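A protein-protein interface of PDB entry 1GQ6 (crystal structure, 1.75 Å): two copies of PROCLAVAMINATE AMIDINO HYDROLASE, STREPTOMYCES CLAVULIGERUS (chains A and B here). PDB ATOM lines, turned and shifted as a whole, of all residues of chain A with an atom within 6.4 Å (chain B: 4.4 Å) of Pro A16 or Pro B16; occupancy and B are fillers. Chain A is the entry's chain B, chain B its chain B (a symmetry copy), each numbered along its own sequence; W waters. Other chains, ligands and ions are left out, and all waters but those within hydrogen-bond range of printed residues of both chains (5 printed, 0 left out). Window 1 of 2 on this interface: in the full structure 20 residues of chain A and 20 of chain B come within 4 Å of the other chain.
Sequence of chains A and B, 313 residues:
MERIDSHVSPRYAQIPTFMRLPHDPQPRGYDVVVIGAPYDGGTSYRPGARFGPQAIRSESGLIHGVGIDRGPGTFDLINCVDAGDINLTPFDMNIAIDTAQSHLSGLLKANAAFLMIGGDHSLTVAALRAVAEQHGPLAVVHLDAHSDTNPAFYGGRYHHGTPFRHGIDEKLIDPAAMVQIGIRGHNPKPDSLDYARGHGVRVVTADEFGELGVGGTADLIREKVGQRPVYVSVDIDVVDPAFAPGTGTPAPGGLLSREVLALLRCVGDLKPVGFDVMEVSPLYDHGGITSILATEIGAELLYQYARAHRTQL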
ATOM      1  N   ALA A  13     -18.329  19.716  22.585  1.00  0.00           N
ATOM      2  CA  ALA A  13     -18.164  19.847  21.135  1.00  0.00           C
ATOM      3  C   ALA A  13     -16.898  19.099  20.696  1.00  0.00           C
ATOM      4  O   ALA A  13     -15.990  18.917  21.496  1.00  0.00           O
ATOM      5  CB  ALA A  13     -18.074  21.324  20.749  1.00  0.00           C
ATOM      6  N   GLN A  14     -16.900  18.642  19.448  1.00  0.00           N
ATOM      7  CA  GLN A  14     -15.833  17.876  18.808  1.00  0.00           C
ATOM      8  C   GLN A  14     -15.843  16.395  19.142  1.00  0.00           C
ATOM      9  O   GLN A  14     -16.484  15.957  20.085  1.00  0.00           O
ATOM     10  CB  GLN A  14     -14.438  18.520  19.006  1.00  0.00           C
ATOM     11  CG  GLN A  14     -14.443  19.990  18.680  1.00  0.00           C
ATOM     12  CD  GLN A  14     -14.933  20.309  17.271  1.00  0.00           C
ATOM     13  OE1 GLN A  14     -14.863  19.460  16.372  1.00  0.00           O
ATOM     14  NE2 GLN A  14     -15.394  21.536  17.069  1.00  0.00           N
ATOM     15  N   ILE A  15     -15.192  15.606  18.297  1.00  0.00           N
ATOM     16  CA  ILE A  15     -15.106  14.193  18.549  1.00  0.00           C
ATOM     17  C   ILE A  15     -14.402  13.979  19.904  1.00  0.00           C
ATOM     18  O   ILE A  15     -13.358  14.569  20.182  1.00  0.00           O
ATOM     19  CB  ILE A  15     -14.375  13.579  17.394  1.00  0.00           C
ATOM     20  CG1 ILE A  15     -15.339  13.557  16.196  1.00  0.00           C
ATOM     21  CG2 ILE A  15     -13.919  12.219  17.720  1.00  0.00           C
ATOM     22  CD1 ILE A  15     -14.661  13.575  14.948  1.00  0.00           C
ATOM     23  N   PRO A  16     -14.972  13.167  20.767  1.00  0.00           N
ATOM     24  CA  PRO A  16     -14.427  13.085  22.115  1.00  0.00           C
ATOM     25  C   PRO A  16     -13.092  12.370  22.226  1.00  0.00           C
ATOM     26  O   PRO A  16     -12.972  11.215  21.808  1.00  0.00           O
ATOM     27  CB  PRO A  16     -15.488  12.296  22.880  1.00  0.00           C
ATOM     28  CG  PRO A  16     -16.173  11.480  21.816  1.00  0.00           C
ATOM     29  CD  PRO A  16     -16.145  12.295  20.579  1.00  0.00           C
ATOM     30  N   THR A  17     -12.109  13.067  22.780  1.00  0.00           N
ATOM     31  CA  THR A  17     -10.868  12.449  23.216  1.00  0.00           C
ATOM     32  C   THR A  17     -10.802  12.619  24.738  1.00  0.00           C
ATOM     33  O   THR A  17     -11.520  13.470  25.323  1.00  0.00           O
ATOM     34  CB  THR A  17      -9.660  13.154  22.572  1.00  0.00           C
ATOM     35  OG1 THR A  17      -9.733  14.552  22.840  1.00  0.00           O
ATOM     36  CG2 THR A  17      -9.746  13.068  21.057  1.00  0.00           C
ATOM     37  N   PHE A  18      -9.888  11.895  25.350  1.00  0.00           N
ATOM     38  CA  PHE A  18      -9.695  11.974  26.771  1.00  0.00           C
ATOM     39  C   PHE A  18      -9.244  13.346  27.216  1.00  0.00           C
ATOM     40  O   PHE A  18      -8.170  13.814  26.845  1.00  0.00           O
ATOM     41  CB  PHE A  18      -8.732  10.913  27.242  1.00  0.00           C
ATOM     42  CG  PHE A  18      -8.670  10.841  28.736  1.00  0.00           C
ATOM     43  CD1 PHE A  18      -9.691  10.232  29.448  1.00  0.00           C
ATOM     44  CD2 PHE A  18      -7.657  11.440  29.423  1.00  0.00           C
ATOM     45  CE1 PHE A  18      -9.670  10.200  30.833  1.00  0.00           C
ATOM     46  CE2 PHE A  18      -7.612  11.386  30.797  1.00  0.00           C
ATOM     47  CZ  PHE A  18      -8.618  10.756  31.507  1.00  0.00           C
ATOM     48  N   ARG A  20     -10.097  16.067  26.201  1.00  0.00           N
ATOM     49  CA  ARG A  20      -9.982  16.936  25.015  1.00  0.00           C
ATOM     50  C   ARG A  20      -8.551  17.053  24.547  1.00  0.00           C
ATOM     51  O   ARG A  20      -8.175  18.010  23.835  1.00  0.00           O
ATOM     52  CB  ARG A  20     -10.576  18.338  25.213  1.00  0.00           C
ATOM     53  CG  ARG A  20     -11.966  18.354  25.852  1.00  0.00           C
ATOM     54  CD  ARG A  20     -12.672  19.686  25.776  1.00  0.00           C
ATOM     55  NE  ARG A  20     -13.231  19.866  24.430  1.00  0.00           N
ATOM     56  CZ  ARG A  20     -13.667  20.993  23.927  1.00  0.00           C
ATOM     57  NH1 ARG A  20     -13.579  22.137  24.610  1.00  0.00           N
ATOM     58  NH2 ARG A  20     -14.184  20.975  22.706  1.00  0.00           N
ATOM     59  N   GLN A  54     -14.917   4.398  25.434  1.00  0.00           N
ATOM     60  CA  GLN A  54     -15.814   5.314  24.727  1.00  0.00           C
ATOM     61  C   GLN A  54     -16.563   6.198  25.733  1.00  0.00           C
ATOM     62  O   GLN A  54     -16.669   7.422  25.581  1.00  0.00           O
ATOM     63  CB  GLN A  54     -16.801   4.509  23.857  1.00  0.00           C
ATOM     64  CG  GLN A  54     -17.623   5.335  22.904  1.00  0.00           C
ATOM     65  CD  GLN A  54     -18.676   4.486  22.176  1.00  0.00           C
ATOM     66  OE1 GLN A  54     -19.707   4.133  22.758  1.00  0.00           O
ATOM     67  NE2 GLN A  54     -18.379   4.104  20.934  1.00  0.00           N
ATOM     68  N   ARG A  57     -14.189   8.655  27.533  1.00  0.00           N
ATOM     69  CA  ARG A  57     -13.909   9.788  26.633  1.00  0.00           C
ATOM     70  C   ARG A  57     -15.082  10.783  26.553  1.00  0.00           C
ATOM     71  O   ARG A  57     -14.890  11.990  26.666  1.00  0.00           O
ATOM     72  CB  ARG A  57     -13.557   9.327  25.224  1.00  0.00           C
ATOM     73  CG  ARG A  57     -12.189   8.726  25.105  1.00  0.00           C
ATOM     74  CD  ARG A  57     -11.798   8.410  23.712  1.00  0.00           C
ATOM     75  NE  ARG A  57     -10.421   7.927  23.641  1.00  0.00           N
ATOM     76  CZ  ARG A  57     -10.091   6.661  23.493  1.00  0.00           C
ATOM     77  NH1 ARG A  57     -11.032   5.734  23.401  1.00  0.00           N
ATOM     78  NH2 ARG A  57      -8.815   6.324  23.436  1.00  0.00           N
ATOM     79  N   SER A  58     -16.276  10.265  26.335  1.00  0.00           N
ATOM     80  CA  SER A  58     -17.460  11.102  26.204  1.00  0.00           C
ATOM     81  C   SER A  58     -17.701  11.990  27.419  1.00  0.00           C
ATOM     82  O   SER A  58     -18.109  13.134  27.264  1.00  0.00           O
ATOM     83  CB  SER A  58     -18.679  10.240  25.963  1.00  0.00           C
ATOM     84  OG  SER A  58     -18.559   9.668  24.655  1.00  0.00           O
ATOM     85  N   GLU A  59     -17.484  11.466  28.611  1.00  0.00           N
ATOM     86  CA  GLU A  59     -17.762  12.247  29.821  1.00  0.00           C
ATOM     87  C   GLU A  59     -16.558  13.089  30.215  1.00  0.00           C
ATOM     88  O   GLU A  59     -16.699  14.063  30.965  1.00  0.00           O
ATOM     89  CB  GLU A  59     -18.183  11.332  30.984  1.00  0.00           C
ATOM     90  CG  GLU A  59     -19.385  10.454  30.708  1.00  0.00           C
ATOM     91  CD  GLU A  59     -20.719  11.166  30.842  1.00  0.00           C
ATOM     92  OE1 GLU A  59     -20.749  12.391  31.126  1.00  0.00           O
ATOM     93  OE2 GLU A  59     -21.739  10.475  30.628  1.00  0.00           O
ATOM     94  N   SER A  60     -15.375  12.740  29.704  1.00  0.00           N
ATOM     95  CA  SER A  60     -14.144  13.442  30.135  1.00  0.00           C
ATOM     96  C   SER A  60     -14.010  14.885  29.718  1.00  0.00           C
ATOM     97  O   SER A  60     -13.194  15.608  30.261  1.00  0.00           O
ATOM     98  CB  SER A  60     -12.884  12.709  29.649  1.00  0.00           C
ATOM     99  OG  SER A  60     -12.749  12.843  28.239  1.00  0.00           O
ATOM    100  N   ASP A  82      -4.057  11.535  23.278  1.00  0.00           N
ATOM    101  CA  ASP A  82      -4.958  10.401  23.256  1.00  0.00           C
ATOM    102  C   ASP A  82      -4.586   9.602  21.993  1.00  0.00           C
ATOM    103  O   ASP A  82      -4.755  10.088  20.882  1.00  0.00           O
ATOM    104  CB  ASP A  82      -6.394  10.895  23.233  1.00  0.00           C
ATOM    105  CG  ASP A  82      -7.409   9.775  23.315  1.00  0.00           C
ATOM    106  OD1 ASP A  82      -7.086   8.648  22.886  1.00  0.00           O
ATOM    107  OD2 ASP A  82      -8.559   9.931  23.767  1.00  0.00           O
ATOM    108  N   GLN B  14     -11.883   2.617  18.813  1.00  0.00           N
ATOM    109  CA  GLN B  14     -11.426   3.905  18.298  1.00  0.00           C
ATOM    110  C   GLN B  14     -12.328   5.073  18.654  1.00  0.00           C
ATOM    111  O   GLN B  14     -13.466   4.901  19.060  1.00  0.00           O
ATOM    112  CB  GLN B  14     -11.088   3.856  16.786  1.00  0.00           C
ATOM    113  CG  GLN B  14     -10.201   2.688  16.444  1.00  0.00           C
ATOM    114  CD  GLN B  14      -8.899   2.649  17.237  1.00  0.00           C
ATOM    115  OE1 GLN B  14      -8.424   3.684  17.725  1.00  0.00           O
ATOM    116  NE2 GLN B  14      -8.304   1.468  17.338  1.00  0.00           N
ATOM    117  N   ILE B  15     -11.772   6.277  18.585  1.00  0.00           N
ATOM    118  CA  ILE B  15     -12.556   7.451  18.862  1.00  0.00           C
ATOM    119  C   ILE B  15     -13.728   7.504  17.861  1.00  0.00           C
ATOM    120  O   ILE B  15     -13.548   7.334  16.656  1.00  0.00           O
ATOM    121  CB  ILE B  15     -11.637   8.631  18.766  1.00  0.00           C
ATOM    122  CG1 ILE B  15     -10.748   8.626  20.022  1.00  0.00           C
ATOM    123  CG2 ILE B  15     -12.397   9.886  18.672  1.00  0.00           C
ATOM    124  CD1 ILE B  15      -9.500   9.269  19.810  1.00  0.00           C
ATOM    125  N   PRO B  16     -14.934   7.706  18.344  1.00  0.00           N
ATOM    126  CA  PRO B  16     -16.076   7.583  17.447  1.00  0.00           C
ATOM    127  C   PRO B  16     -16.222   8.707  16.436  1.00  0.00           C
ATOM    128  O   PRO B  16     -16.294   9.878  16.818  1.00  0.00           O
ATOM    129  CB  PRO B  16     -17.274   7.597  18.395  1.00  0.00           C
ATOM    130  CG  PRO B  16     -16.777   8.349  19.601  1.00  0.00           C
ATOM    131  CD  PRO B  16     -15.333   8.039  19.724  1.00  0.00           C
ATOM    132  N   THR B  17     -16.256   8.335  15.164  1.00  0.00           N
ATOM    133  CA  THR B  17     -16.671   9.237  14.102  1.00  0.00           C
ATOM    134  C   THR B  17     -17.954   8.649  13.501  1.00  0.00           C
ATOM    135  O   THR B  17     -18.262   7.445  13.695  1.00  0.00           O
ATOM    136  CB  THR B  17     -15.588   9.317  13.010  1.00  0.00           C
ATOM    137  OG1 THR B  17     -15.275   8.002  12.560  1.00  0.00           O
ATOM    138  CG2 THR B  17     -14.282   9.822  13.601  1.00  0.00           C
ATOM    139  N   ARG B  57     -22.682   9.829  16.856  1.00  0.00           N
ATOM    140  CA  ARG B  57     -21.366   9.243  16.546  1.00  0.00           C
ATOM    141  C   ARG B  57     -21.103   7.935  17.316  1.00  0.00           C
ATOM    142  O   ARG B  57     -20.680   6.940  16.737  1.00  0.00           O
ATOM    143  CB  ARG B  57     -20.226  10.216  16.825  1.00  0.00           C
ATOM    144  CG  ARG B  57     -20.114  11.325  15.822  1.00  0.00           C
ATOM    145  CD  ARG B  57     -18.923  12.183  16.017  1.00  0.00           C
ATOM    146  NE  ARG B  57     -18.805  13.180  14.955  1.00  0.00           N
ATOM    147  CZ  ARG B  57     -19.126  14.448  15.095  1.00  0.00           C
ATOM    148  NH1 ARG B  57     -19.591  14.893  16.253  1.00  0.00           N
ATOM    149  NH2 ARG B  57     -18.979  15.274  14.075  1.00  0.00           N
ATOM    150  N   SER B  58     -21.336   7.964  18.614  1.00  0.00           N
ATOM    151  CA  SER B  58     -21.095   6.804  19.460  1.00  0.00           C
ATOM    152  C   SER B  58     -21.867   5.568  19.012  1.00  0.00           C
ATOM    153  O   SER B  58     -21.339   4.465  19.077  1.00  0.00           O
ATOM    154  CB  SER B  58     -21.450   7.125  20.894  1.00  0.00           C
ATOM    155  OG  SER B  58     -20.489   8.069  21.383  1.00  0.00           O
HETATM  156  O   HOH W   1     -13.797   5.789  22.176  1.00  0.00           O
HETATM  157  O   HOH W   2     -22.211   3.023  21.746  1.00  0.00           O
HETATM  158  O   HOH W   3     -15.971   4.167  19.328  1.00  0.00           O
HETATM  159  O   HOH W   4     -18.974  14.101  19.107  1.00  0.00           O
HETATM  160  O   HOH W   5     -19.644   2.129  19.033  1.00  0.00           O
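Hydrophobic or aromatic side chains of chain A that line the printed part of chain B: Ile A15 and Pro A16.
Of the 6 printed residues of chain B, 4 touch a printed residue of chain A.
Hydrophobic or aromatic side chains of chain B that line the printed part of chain A: Ile B15 and Pro B16.
Among the printed residues, no Asp or Glu carboxylate lies within 4 Å of a Lys or Arg side-chain nitrogen of the other chain.
Ile A15 touches its own counterpart, Ile B15.
Ile A15 touches Pro B16, and with the chains exchanged Pro A16 touches Ile B15.
Ile A15 touches Arg B57, and with the chains exchanged Arg A57 touches Ile B15.
Pro A16 touches its own counterpart, Pro B16.
Positions printed for both chains: 14, 15, 16, 17, 57 and 58.
Ile B15 touches Ile A15 (CG2 to CG2, 2.9 Å).
Ile A15 touches Pro B16 (CG2 to O, 3.5 Å).
Ile A15 touches Arg B57.
CG2 of Ile B15 touches O of Pro A16, at 3.5 Å.
Pro A16 touches Pro B16.
Gln A54 touches Ser B58.
Arg A57 touches Ile B15 (NE to CG1, 3.7 Å).
OD1 of Asp A82 touches CD1 of Ile B15 (3.96 Å).
Of chain B, only Ile B15 and Pro B16 come within 4 Å of Pro A16.
Arg A20 touches none of the printed residues of chain B.
Of the printed residues of chain B, Gln A54 touches Ser B58 (3.5 Å).
Ser A60 touches none of the printed residues of chain B.
Of the printed residues of chain B, Asp A82 touches Ile B15 (3.96 Å).
Pro B16 touches just these residues of chain A: Ile A15 and Pro A16.
Of the printed residues of chain A, Ser B58 touches Gln A54.
The nearest residue of chain A that does not touch Pro B16 is Gln A54 (4.5 Å).
The nearest printed residue of chain A that does not touch Arg B57 is Gln A14 (5.0 Å).
Water W3 lies within hydrogen-bond range of the backbone carbonyl oxygen (O) of Gln B14 (2.6 Å) and the side-chain amide nitrogen (NE2) of Gln A54 (2.9 Å).
Water W5 bridges O of Ser B58 and NE2 of Gln A54.
Water W2 bridges OE1 of Gln A54 and O of Ser B58.
Water W4 lies within hydrogen-bond range of NH1 of Arg B57 (3.0 Å) and O of Gln A14 (3.3 Å).
Water W1 lies within hydrogen-bond range of the guanidinium group of Arg A57 (3.0 Å) and the backbone carbonyl oxygen of Gln B14 (3.3 Å).
N of Phe A18 sits at hydrogen-bond distance from OD2 of Asp A82 (2.9 Å).
The backbone carbonyl oxygen (O) of Gln A54 sits at hydrogen-bond distance from the side-chain hydroxyl (OG) of Ser A58, 3.1 Å away.
The backbone carbonyl oxygen (O) of Arg A57 sits at hydrogen-bond distance from the side-chain hydroxyl (OG) of Ser A60, at 2.8 Å.
NE of Arg A57 lies within salt-bridge range of OD2 of Asp A82, at 2.7 Å.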
